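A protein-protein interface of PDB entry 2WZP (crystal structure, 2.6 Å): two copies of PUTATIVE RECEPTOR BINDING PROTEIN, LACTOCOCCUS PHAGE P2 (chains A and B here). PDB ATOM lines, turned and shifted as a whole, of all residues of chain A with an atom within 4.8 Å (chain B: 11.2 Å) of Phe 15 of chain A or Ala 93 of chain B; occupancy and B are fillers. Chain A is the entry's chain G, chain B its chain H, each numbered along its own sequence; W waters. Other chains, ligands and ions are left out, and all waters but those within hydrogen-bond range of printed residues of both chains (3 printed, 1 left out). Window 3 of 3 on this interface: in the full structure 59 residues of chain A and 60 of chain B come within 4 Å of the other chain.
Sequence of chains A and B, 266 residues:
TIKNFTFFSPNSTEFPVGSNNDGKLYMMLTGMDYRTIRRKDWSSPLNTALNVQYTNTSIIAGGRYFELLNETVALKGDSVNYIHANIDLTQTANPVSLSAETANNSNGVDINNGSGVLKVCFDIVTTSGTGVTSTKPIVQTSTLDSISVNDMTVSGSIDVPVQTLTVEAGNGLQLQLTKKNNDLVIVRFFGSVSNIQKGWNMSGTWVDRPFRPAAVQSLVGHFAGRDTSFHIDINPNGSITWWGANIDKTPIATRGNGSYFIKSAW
Water W2 bridges the backbone carbonyl oxygen of Val 96 of chain B (2.7 Å) and the side-chain amide oxygen of Asn 4 of chain A (2.8 Å).
Water W1 lies within hydrogen-bond range of O of Thr 92 of chain B and O of Phe 8 of chain A.
Water W3 lies within hydrogen-bond range of the backbone NH (N) of Phe 8 of chain A (3.0 Å), the side-chain hydroxyl (OG) of Ser 19 of chain B (3.2 Å) and the guanidinium group (NH1) of Arg 64 of chain B (3.5 Å).
Position printed for both chains: 17.
Of the 16 pairs that touch across the chains among the printed residues, none has its exchanged pair printed and touching as well.
O of Tyr 65 of chain B sits at hydrogen-bond distance from N of Phe 5 of chain A (3.2 Å).
The backbone NH (N) of Phe 8 of chain A lies within hydrogen-bond range of the side-chain hydroxyl (OG) of Ser 19 of chain B (3.3 Å).
Among the printed residues, pairs that only touch across the chains: Asn 4 of chain A with Phe 66 of chain B (3.6 Å), Asn 4 of chain A with Pro 95 of chain B (3.5 Å), Asn 4 of chain A with Val 96 of chain B (3.3 Å), Phe 5 of chain A with Glu 67 of chain B (3.5 Å), Phe 7 of chain A with Ser 19 of chain B (3.8 Å), Phe 7 of chain A with Arg 64 of chain B (3.6 Å), Phe 7 of chain A with Tyr 65 of chain B (3.9 Å), Phe 7 of chain A with Ile 87 of chain B (3.7 Å), Phe 7 of chain A with Leu 89 of chain B (3.8 Å), Phe 7 of chain A with Pro 95 of chain B (3.4 Å), Phe 7 of chain A with Val 96 of chain B (3.4 Å), Phe 8 of chain A with Thr 92 of chain B (3.5 Å), Phe 15 of chain A with Thr 92 of chain B (3.3 Å) and Phe 15 of chain A with Ala 93 of chain B (3.4 Å).
Phe 15 of chain A touches just these residues of chain B: Thr 92 (3.3 Å) and Ala 93 (3.4 Å).
Of chain A, only Phe 15 comes within 4 Å of Ala 93 of chain B.
No residue of chain B comes within 4 Å of Ser 9 of chain A.
Glu 14 of chain A touches none of the printed residues of chain B.
No residue of chain B comes within 4 Å of Pro 16 of chain A.
Val 17 of chain A touches none of the printed residues of chain B.
Of the printed residues of chain A, Pro 95 of chain B touches Asn 4 (3.5 Å) and Phe 7 (3.4 Å).
Of the printed residues of chain A, Leu 89 of chain B touches Phe 7 (3.8 Å).
Thr 90 of chain B touches none of the printed residues of chain A.
Asn 94 of chain B touches none of the printed residues of chain A.
The nearest residue of chain B that does not touch Phe 15 of chain A is Pro 95 of chain B (4.05 Å).
The nearest printed residue of chain A that does not touch Ala 93 of chain B is Asn 4 of chain A (4.8 Å).
The nearest printed residue of chain A that does not touch Tyr 65 of chain B is Asn 4 of chain A (4.2 Å).
Of the 10 printed residues of chain A, 5 touch a printed residue of chain B.
Along chain A the printed residues that touch a printed residue of chain B span positions 4 to 15.
Among the printed residues, no Asp or Glu carboxylate lies within 4 Å of a Lys or Arg side-chain nitrogen of the other chain.
OG of Ser 9 of chain A lies within hydrogen-bond range of N of Phe 15 of chain A (3.0 Å).
The side-chain carboxylate (OE1) of Glu 67 of chain B is in hydrogen-bond range of the side-chain hydroxyl (OH) of Tyr 65 of chain B (2.6 Å).
N of Asp 88 of chain B is in hydrogen-bond range of O of Pro 95 of chain B (2.8 Å).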
ATOM      1  N   ASN A   4       5.525  25.086   7.163  1.00  0.00           N
ATOM      2  CA  ASN A   4       5.879  23.863   7.890  1.00  0.00           C
ATOM      3  C   ASN A   4       5.966  24.078   9.366  1.00  0.00           C
ATOM      4  O   ASN A   4       6.431  25.130   9.799  1.00  0.00           O
ATOM      5  CB  ASN A   4       7.180  23.278   7.364  1.00  0.00           C
ATOM      6  CG  ASN A   4       7.132  22.998   5.894  1.00  0.00           C
ATOM      7  OD1 ASN A   4       7.855  23.598   5.108  1.00  0.00           O
ATOM      8  ND2 ASN A   4       6.179  22.198   5.479  1.00  0.00           N
ATOM      9  N   PHE A   5       5.512  23.080  10.152  1.00  0.00           N
ATOM     10  CA  PHE A   5       5.504  23.181  11.597  1.00  0.00           C
ATOM     11  C   PHE A   5       6.215  22.064  12.288  1.00  0.00           C
ATOM     12  O   PHE A   5       7.186  22.362  12.970  1.00  0.00           O
ATOM     13  CB  PHE A   5       4.082  23.393  12.135  1.00  0.00           C
ATOM     14  CG  PHE A   5       3.469  24.676  11.640  1.00  0.00           C
ATOM     15  CD1 PHE A   5       2.697  24.692  10.484  1.00  0.00           C
ATOM     16  CD2 PHE A   5       3.729  25.886  12.287  1.00  0.00           C
ATOM     17  CE1 PHE A   5       2.211  25.890   9.977  1.00  0.00           C
ATOM     18  CE2 PHE A   5       3.240  27.081  11.776  1.00  0.00           C
ATOM     19  CZ  PHE A   5       2.482  27.072  10.630  1.00  0.00           C
ATOM     20  N   PHE A   7       8.656  20.178  12.035  1.00  0.00           N
ATOM     21  CA  PHE A   7       9.964  19.998  11.381  1.00  0.00           C
ATOM     22  C   PHE A   7      11.020  20.721  12.167  1.00  0.00           C
ATOM     23  O   PHE A   7      10.721  21.731  12.800  1.00  0.00           O
ATOM     24  CB  PHE A   7       9.926  20.504   9.913  1.00  0.00           C
ATOM     25  CG  PHE A   7       8.893  19.785   9.072  1.00  0.00           C
ATOM     26  CD1 PHE A   7       7.595  20.275   8.968  1.00  0.00           C
ATOM     27  CD2 PHE A   7       9.198  18.577   8.440  1.00  0.00           C
ATOM     28  CE1 PHE A   7       6.629  19.590   8.223  1.00  0.00           C
ATOM     29  CE2 PHE A   7       8.231  17.900   7.692  1.00  0.00           C
ATOM     30  CZ  PHE A   7       6.947  18.398   7.618  1.00  0.00           C
ATOM     31  N   PHE A   8      12.240  20.188  12.163  1.00  0.00           N
ATOM     32  CA  PHE A   8      13.335  20.771  12.921  1.00  0.00           C
ATOM     33  C   PHE A   8      13.835  22.074  12.305  1.00  0.00           C
ATOM     34  O   PHE A   8      13.808  22.233  11.085  1.00  0.00           O
ATOM     35  CB  PHE A   8      14.423  19.729  13.229  1.00  0.00           C
ATOM     36  CG  PHE A   8      15.695  19.795  12.427  1.00  0.00           C
ATOM     37  CD1 PHE A   8      16.768  20.578  12.851  1.00  0.00           C
ATOM     38  CD2 PHE A   8      15.843  19.047  11.274  1.00  0.00           C
ATOM     39  CE1 PHE A   8      17.944  20.629  12.112  1.00  0.00           C
ATOM     40  CE2 PHE A   8      17.018  19.109  10.537  1.00  0.00           C
ATOM     41  CZ  PHE A   8      18.052  19.907  10.951  1.00  0.00           C
ATOM     42  N   SER A   9      14.185  23.038  13.161  1.00  0.00           N
ATOM     43  CA  SER A   9      14.649  24.352  12.747  1.00  0.00           C
ATOM     44  C   SER A   9      16.170  24.334  12.925  1.00  0.00           C
ATOM     45  O   SER A   9      16.645  24.390  14.068  1.00  0.00           O
ATOM     46  CB  SER A   9      13.985  25.436  13.591  1.00  0.00           C
ATOM     47  OG  SER A   9      12.585  25.443  13.366  1.00  0.00           O
ATOM     48  N   THR A  13      15.153  29.058  14.263  1.00  0.00           N
ATOM     49  CA  THR A  13      14.249  30.139  13.852  1.00  0.00           C
ATOM     50  C   THR A  13      13.322  29.850  12.668  1.00  0.00           C
ATOM     51  O   THR A  13      12.365  30.593  12.454  1.00  0.00           O
ATOM     52  CB  THR A  13      15.076  31.386  13.538  1.00  0.00           C
ATOM     53  OG1 THR A  13      15.965  31.109  12.441  1.00  0.00           O
ATOM     54  CG2 THR A  13      15.842  31.887  14.747  1.00  0.00           C
ATOM     55  N   GLU A  14      13.628  28.829  11.876  1.00  0.00           N
ATOM     56  CA  GLU A  14      12.911  28.480  10.643  1.00  0.00           C
ATOM     57  C   GLU A  14      11.413  28.213  10.758  1.00  0.00           C
ATOM     58  O   GLU A  14      10.637  28.808  10.006  1.00  0.00           O
ATOM     59  CB  GLU A  14      13.621  27.329   9.892  1.00  0.00           C
ATOM     60  CG  GLU A  14      14.987  27.710   9.346  1.00  0.00           C
ATOM     61  CD  GLU A  14      16.189  27.580  10.271  1.00  0.00           C
ATOM     62  OE1 GLU A  14      16.007  27.445  11.504  1.00  0.00           O
ATOM     63  OE2 GLU A  14      17.327  27.608   9.753  1.00  0.00           O
ATOM     64  N   PHE A  15      11.006  27.292  11.659  1.00  0.00           N
ATOM     65  CA  PHE A  15       9.609  26.887  11.771  1.00  0.00           C
ATOM     66  C   PHE A  15       8.985  27.098  13.148  1.00  0.00           C
ATOM     67  O   PHE A  15       8.752  26.117  13.866  1.00  0.00           O
ATOM     68  CB  PHE A  15       9.426  25.438  11.244  1.00  0.00           C
ATOM     69  CG  PHE A  15      10.134  25.144   9.941  1.00  0.00           C
ATOM     70  CD1 PHE A  15       9.745  25.775   8.759  1.00  0.00           C
ATOM     71  CD2 PHE A  15      11.220  24.280   9.898  1.00  0.00           C
ATOM     72  CE1 PHE A  15      10.427  25.532   7.554  1.00  0.00           C
ATOM     73  CE2 PHE A  15      11.900  24.049   8.699  1.00  0.00           C
ATOM     74  CZ  PHE A  15      11.498  24.679   7.536  1.00  0.00           C
ATOM     75  N   PRO A  16       8.698  28.357  13.557  1.00  0.00           N
ATOM     76  CA  PRO A  16       8.047  28.571  14.875  1.00  0.00           C
ATOM     77  C   PRO A  16       6.620  28.043  14.896  1.00  0.00           C
ATOM     78  O   PRO A  16       5.895  28.166  13.912  1.00  0.00           O
ATOM     79  CB  PRO A  16       8.088  30.082  15.066  1.00  0.00           C
ATOM     80  CG  PRO A  16       8.269  30.636  13.740  1.00  0.00           C
ATOM     81  CD  PRO A  16       8.940  29.638  12.864  1.00  0.00           C
ATOM     82  N   VAL A  17       6.231  27.390  15.992  1.00  0.00           N
ATOM     83  CA  VAL A  17       4.876  26.865  16.027  1.00  0.00           C
ATOM     84  C   VAL A  17       3.950  27.741  16.856  1.00  0.00           C
ATOM     85  O   VAL A  17       4.165  27.925  18.051  1.00  0.00           O
ATOM     86  CB  VAL A  17       4.684  25.310  16.128  1.00  0.00           C
ATOM     87  CG1 VAL A  17       5.992  24.557  16.291  1.00  0.00           C
ATOM     88  CG2 VAL A  17       3.654  24.903  17.151  1.00  0.00           C
ATOM     89  N   VAL B  17      12.302  17.769  22.778  1.00  0.00           N
ATOM     90  CA  VAL B  17      11.414  17.019  21.915  1.00  0.00           C
ATOM     91  C   VAL B  17      11.716  17.233  20.429  1.00  0.00           C
ATOM     92  O   VAL B  17      11.661  18.359  19.927  1.00  0.00           O
ATOM     93  CB  VAL B  17       9.920  16.954  22.369  1.00  0.00           C
ATOM     94  CG1 VAL B  17       9.621  17.795  23.614  1.00  0.00           C
ATOM     95  CG2 VAL B  17       8.955  17.238  21.253  1.00  0.00           C
ATOM     96  N   GLY B  18      12.117  16.155  19.771  1.00  0.00           N
ATOM     97  CA  GLY B  18      12.411  16.162  18.348  1.00  0.00           C
ATOM     98  C   GLY B  18      11.140  16.156  17.525  1.00  0.00           C
ATOM     99  O   GLY B  18      10.064  15.742  18.003  1.00  0.00           O
ATOM    100  N   SER B  19      11.256  16.620  16.269  1.00  0.00           N
ATOM    101  CA  SER B  19      10.103  16.664  15.376  1.00  0.00           C
ATOM    102  C   SER B  19       9.588  15.252  15.053  1.00  0.00           C
ATOM    103  O   SER B  19       8.380  15.061  14.932  1.00  0.00           O
ATOM    104  CB  SER B  19      10.414  17.494  14.138  1.00  0.00           C
ATOM    105  OG  SER B  19      11.722  17.243  13.653  1.00  0.00           O
ATOM    106  N   ASP B  22       7.525  13.959  18.170  1.00  0.00           N
ATOM    107  CA  ASP B  22       6.173  14.506  18.135  1.00  0.00           C
ATOM    108  C   ASP B  22       5.369  13.878  16.992  1.00  0.00           C
ATOM    109  O   ASP B  22       4.203  13.550  17.190  1.00  0.00           O
ATOM    110  CB  ASP B  22       6.180  16.034  18.095  1.00  0.00           C
ATOM    111  CG  ASP B  22       6.031  16.666  19.484  1.00  0.00           C
ATOM    112  OD1 ASP B  22       5.932  15.907  20.486  1.00  0.00           O
ATOM    113  OD2 ASP B  22       5.939  17.914  19.565  1.00  0.00           O
ATOM    114  N   TYR B  26       1.878  12.054  17.639  1.00  0.00           N
ATOM    115  CA  TYR B  26       0.663  12.451  16.936  1.00  0.00           C
ATOM    116  C   TYR B  26       0.036  11.304  16.181  1.00  0.00           C
ATOM    117  O   TYR B  26      -1.175  11.111  16.262  1.00  0.00           O
ATOM    118  CB  TYR B  26       0.931  13.642  16.029  1.00  0.00           C
ATOM    119  CG  TYR B  26       1.399  14.881  16.761  1.00  0.00           C
ATOM    120  CD1 TYR B  26       0.986  15.146  18.071  1.00  0.00           C
ATOM    121  CD2 TYR B  26       2.178  15.836  16.119  1.00  0.00           C
ATOM    122  CE1 TYR B  26       1.371  16.311  18.726  1.00  0.00           C
ATOM    123  CE2 TYR B  26       2.588  16.987  16.772  1.00  0.00           C
ATOM    124  CZ  TYR B  26       2.161  17.232  18.067  1.00  0.00           C
ATOM    125  OH  TYR B  26       2.540  18.386  18.703  1.00  0.00           O
ATOM    126  N   ARG B  64       3.403  14.731  10.817  1.00  0.00           N
ATOM    127  CA  ARG B  64       3.964  16.063  10.564  1.00  0.00           C
ATOM    128  C   ARG B  64       2.903  16.987  10.057  1.00  0.00           C
ATOM    129  O   ARG B  64       2.237  16.675   9.070  1.00  0.00           O
ATOM    130  CB  ARG B  64       5.125  16.012   9.567  1.00  0.00           C
ATOM    131  CG  ARG B  64       6.171  14.938   9.856  1.00  0.00           C
ATOM    132  CD  ARG B  64       6.777  15.072  11.228  1.00  0.00           C
ATOM    133  NE  ARG B  64       7.912  14.170  11.363  1.00  0.00           N
ATOM    134  CZ  ARG B  64       9.179  14.525  11.184  1.00  0.00           C
ATOM    135  NH1 ARG B  64       9.488  15.780  10.892  1.00  0.00           N
ATOM    136  NH2 ARG B  64      10.149  13.628  11.310  1.00  0.00           N
ATOM    137  N   TYR B  65       2.714  18.115  10.764  1.00  0.00           N
ATOM    138  CA  TYR B  65       1.715  19.130  10.448  1.00  0.00           C
ATOM    139  C   TYR B  65       2.283  20.228   9.579  1.00  0.00           C
ATOM    140  O   TYR B  65       3.349  20.776   9.857  1.00  0.00           O
ATOM    141  CB  TYR B  65       1.109  19.712  11.721  1.00  0.00           C
ATOM    142  CG  TYR B  65       0.089  20.804  11.480  1.00  0.00           C
ATOM    143  CD1 TYR B  65      -1.264  20.505  11.350  1.00  0.00           C
ATOM    144  CD2 TYR B  65       0.462  22.144  11.474  1.00  0.00           C
ATOM    145  CE1 TYR B  65      -2.211  21.508  11.147  1.00  0.00           C
ATOM    146  CE2 TYR B  65      -0.469  23.156  11.244  1.00  0.00           C
ATOM    147  CZ  TYR B  65      -1.807  22.832  11.072  1.00  0.00           C
ATOM    148  OH  TYR B  65      -2.727  23.825  10.836  1.00  0.00           O
ATOM    149  N   PHE B  66       1.536  20.575   8.542  1.00  0.00           N
ATOM    150  CA  PHE B  66       1.877  21.663   7.640  1.00  0.00           C
ATOM    151  C   PHE B  66       0.614  22.249   7.042  1.00  0.00           C
ATOM    152  O   PHE B  66      -0.449  21.618   7.071  1.00  0.00           O
ATOM    153  CB  PHE B  66       2.875  21.241   6.560  1.00  0.00           C
ATOM    154  CG  PHE B  66       2.444  20.073   5.710  1.00  0.00           C
ATOM    155  CD1 PHE B  66       1.807  20.279   4.492  1.00  0.00           C
ATOM    156  CD2 PHE B  66       2.709  18.761   6.112  1.00  0.00           C
ATOM    157  CE1 PHE B  66       1.406  19.193   3.709  1.00  0.00           C
ATOM    158  CE2 PHE B  66       2.323  17.673   5.320  1.00  0.00           C
ATOM    159  CZ  PHE B  66       1.685  17.896   4.119  1.00  0.00           C
ATOM    160  N   GLU B  67       0.730  23.470   6.535  1.00  0.00           N
ATOM    161  CA  GLU B  67      -0.369  24.231   5.968  1.00  0.00           C
ATOM    162  C   GLU B  67      -0.092  24.654   4.530  1.00  0.00           C
ATOM    163  O   GLU B  67       1.011  25.114   4.197  1.00  0.00           O
ATOM    164  CB  GLU B  67      -0.627  25.472   6.817  1.00  0.00           C
ATOM    165  CG  GLU B  67      -1.056  25.137   8.230  1.00  0.00           C
ATOM    166  CD  GLU B  67      -1.203  26.316   9.161  1.00  0.00           C
ATOM    167  OE1 GLU B  67      -1.792  26.138  10.251  1.00  0.00           O
ATOM    168  OE2 GLU B  67      -0.697  27.408   8.818  1.00  0.00           O
ATOM    169  N   ASN B  86       4.657  15.229  -0.389  1.00  0.00           N
ATOM    170  CA  ASN B  86       5.950  14.547  -0.366  1.00  0.00           C
ATOM    171  C   ASN B  86       6.826  15.165   0.703  1.00  0.00           C
ATOM    172  O   ASN B  86       7.001  16.385   0.732  1.00  0.00           O
ATOM    173  CB  ASN B  86       6.617  14.612  -1.738  1.00  0.00           C
ATOM    174  CG  ASN B  86       5.727  14.172  -2.860  1.00  0.00           C
ATOM    175  OD1 ASN B  86       5.343  13.005  -2.946  1.00  0.00           O
ATOM    176  ND2 ASN B  86       5.391  15.099  -3.743  1.00  0.00           N
ATOM    177  N   ILE B  87       7.344  14.317   1.613  1.00  0.00           N
ATOM    178  CA  ILE B  87       8.157  14.775   2.730  1.00  0.00           C
ATOM    179  C   ILE B  87       9.570  14.266   2.651  1.00  0.00           C
ATOM    180  O   ILE B  87       9.804  13.064   2.745  1.00  0.00           O
ATOM    181  CB  ILE B  87       7.505  14.561   4.115  1.00  0.00           C
ATOM    182  CG1 ILE B  87       6.069  15.156   4.143  1.00  0.00           C
ATOM    183  CG2 ILE B  87       8.376  15.198   5.210  1.00  0.00           C
ATOM    184  CD1 ILE B  87       5.210  14.671   5.269  1.00  0.00           C
ATOM    185  N   ASP B  88      10.521  15.199   2.486  1.00  0.00           N
ATOM    186  CA  ASP B  88      11.943  14.879   2.420  1.00  0.00           C
ATOM    187  C   ASP B  88      12.639  15.676   3.496  1.00  0.00           C
ATOM    188  O   ASP B  88      12.865  16.878   3.354  1.00  0.00           O
ATOM    189  CB  ASP B  88      12.517  15.178   1.036  1.00  0.00           C
ATOM    190  CG  ASP B  88      13.969  14.772   0.830  1.00  0.00           C
ATOM    191  OD1 ASP B  88      14.634  14.362   1.826  1.00  0.00           O
ATOM    192  OD2 ASP B  88      14.444  14.866  -0.313  1.00  0.00           O
ATOM    193  N   LEU B  89      12.960  15.004   4.590  1.00  0.00           N
ATOM    194  CA  LEU B  89      13.558  15.637   5.765  1.00  0.00           C
ATOM    195  C   LEU B  89      14.945  16.210   5.549  1.00  0.00           C
ATOM    196  O   LEU B  89      15.359  17.079   6.312  1.00  0.00           O
ATOM    197  CB  LEU B  89      13.501  14.722   6.997  1.00  0.00           C
ATOM    198  CG  LEU B  89      12.117  14.226   7.393  1.00  0.00           C
ATOM    199  CD1 LEU B  89      12.217  13.294   8.568  1.00  0.00           C
ATOM    200  CD2 LEU B  89      11.175  15.373   7.691  1.00  0.00           C
ATOM    201  N   THR B  90      15.641  15.769   4.497  1.00  0.00           N
ATOM    202  CA  THR B  90      16.985  16.259   4.157  1.00  0.00           C
ATOM    203  C   THR B  90      16.924  17.668   3.548  1.00  0.00           C
ATOM    204  O   THR B  90      17.904  18.412   3.607  1.00  0.00           O
ATOM    205  CB  THR B  90      17.705  15.294   3.255  1.00  0.00           C
ATOM    206  OG1 THR B  90      17.060  15.321   1.990  1.00  0.00           O
ATOM    207  CG2 THR B  90      17.747  13.875   3.836  1.00  0.00           C
ATOM    208  N   GLN B  91      15.761  18.035   2.984  1.00  0.00           N
ATOM    209  CA  GLN B  91      15.525  19.358   2.436  1.00  0.00           C
ATOM    210  C   GLN B  91      15.086  20.198   3.643  1.00  0.00           C
ATOM    211  O   GLN B  91      13.914  20.529   3.768  1.00  0.00           O
ATOM    212  CB  GLN B  91      14.436  19.289   1.355  1.00  0.00           C
ATOM    213  CG  GLN B  91      14.788  18.479   0.098  1.00  0.00           C
ATOM    214  CD  GLN B  91      16.092  18.902  -0.550  1.00  0.00           C
ATOM    215  OE1 GLN B  91      17.130  18.262  -0.316  1.00  0.00           O
ATOM    216  NE2 GLN B  91      16.099  20.033  -1.270  1.00  0.00           N
ATOM    217  N   THR B  92      16.019  20.488   4.566  1.00  0.00           N
ATOM    218  CA  THR B  92      15.744  21.181   5.818  1.00  0.00           C
ATOM    219  C   THR B  92      14.969  22.486   5.746  1.00  0.00           C
ATOM    220  O   THR B  92      14.147  22.748   6.628  1.00  0.00           O
ATOM    221  CB  THR B  92      16.970  21.206   6.738  1.00  0.00           C
ATOM    222  OG1 THR B  92      18.032  21.951   6.155  1.00  0.00           O
ATOM    223  CG2 THR B  92      17.458  19.804   7.135  1.00  0.00           C
ATOM    224  N   ALA B  93      15.204  23.294   4.712  1.00  0.00           N
ATOM    225  CA  ALA B  93      14.512  24.576   4.537  1.00  0.00           C
ATOM    226  C   ALA B  93      13.089  24.446   3.980  1.00  0.00           C
ATOM    227  O   ALA B  93      12.252  25.296   4.262  1.00  0.00           O
ATOM    228  CB  ALA B  93      15.333  25.499   3.657  1.00  0.00           C
ATOM    229  N   ASN B  94      12.826  23.415   3.167  1.00  0.00           N
ATOM    230  CA  ASN B  94      11.531  23.159   2.501  1.00  0.00           C
ATOM    231  C   ASN B  94      11.258  21.636   2.509  1.00  0.00           C
ATOM    232  O   ASN B  94      11.423  20.998   1.461  1.00  0.00           O
ATOM    233  CB  ASN B  94      11.613  23.658   1.025  1.00  0.00           C
ATOM    234  CG  ASN B  94      11.960  25.117   0.897  1.00  0.00           C
ATOM    235  OD1 ASN B  94      11.108  26.016   1.053  1.00  0.00           O
ATOM    236  ND2 ASN B  94      13.233  25.383   0.638  1.00  0.00           N
ATOM    237  N   PRO B  95      10.935  21.013   3.671  1.00  0.00           N
ATOM    238  CA  PRO B  95      10.802  19.536   3.698  1.00  0.00           C
ATOM    239  C   PRO B  95       9.578  18.970   2.995  1.00  0.00           C
ATOM    240  O   PRO B  95       9.516  17.772   2.758  1.00  0.00           O
ATOM    241  CB  PRO B  95      10.809  19.210   5.189  1.00  0.00           C
ATOM    242  CG  PRO B  95      10.294  20.440   5.842  1.00  0.00           C
ATOM    243  CD  PRO B  95      10.757  21.595   5.020  1.00  0.00           C
ATOM    244  N   VAL B  96       8.602  19.819   2.678  1.00  0.00           N
ATOM    245  CA  VAL B  96       7.342  19.410   2.058  1.00  0.00           C
ATOM    246  C   VAL B  96       7.160  20.017   0.679  1.00  0.00           C
ATOM    247  O   VAL B  96       7.412  21.208   0.483  1.00  0.00           O
ATOM    248  CB  VAL B  96       6.112  19.725   2.975  1.00  0.00           C
ATOM    249  CG1 VAL B  96       4.809  19.224   2.349  1.00  0.00           C
ATOM    250  CG2 VAL B  96       6.295  19.104   4.355  1.00  0.00           C
ATOM    251  N   SER B  97       6.649  19.214  -0.249  1.00  0.00           N
ATOM    252  CA  SER B  97       6.308  19.647  -1.600  1.00  0.00           C
ATOM    253  C   SER B  97       5.070  18.881  -2.081  1.00  0.00           C
ATOM    254  O   SER B  97       4.761  17.794  -1.571  1.00  0.00           O
ATOM    255  CB  SER B  97       7.477  19.429  -2.553  1.00  0.00           C
ATOM    256  OG  SER B  97       7.797  18.048  -2.672  1.00  0.00           O
HETATM  257  O   HOH W   1      13.318  21.026   8.534  1.00  0.00           O
HETATM  258  O   HOH W   2       8.129  22.852   2.468  1.00  0.00           O
HETATM  259  O   HOH W   3      12.355  17.699  10.550  1.00  0.00           O
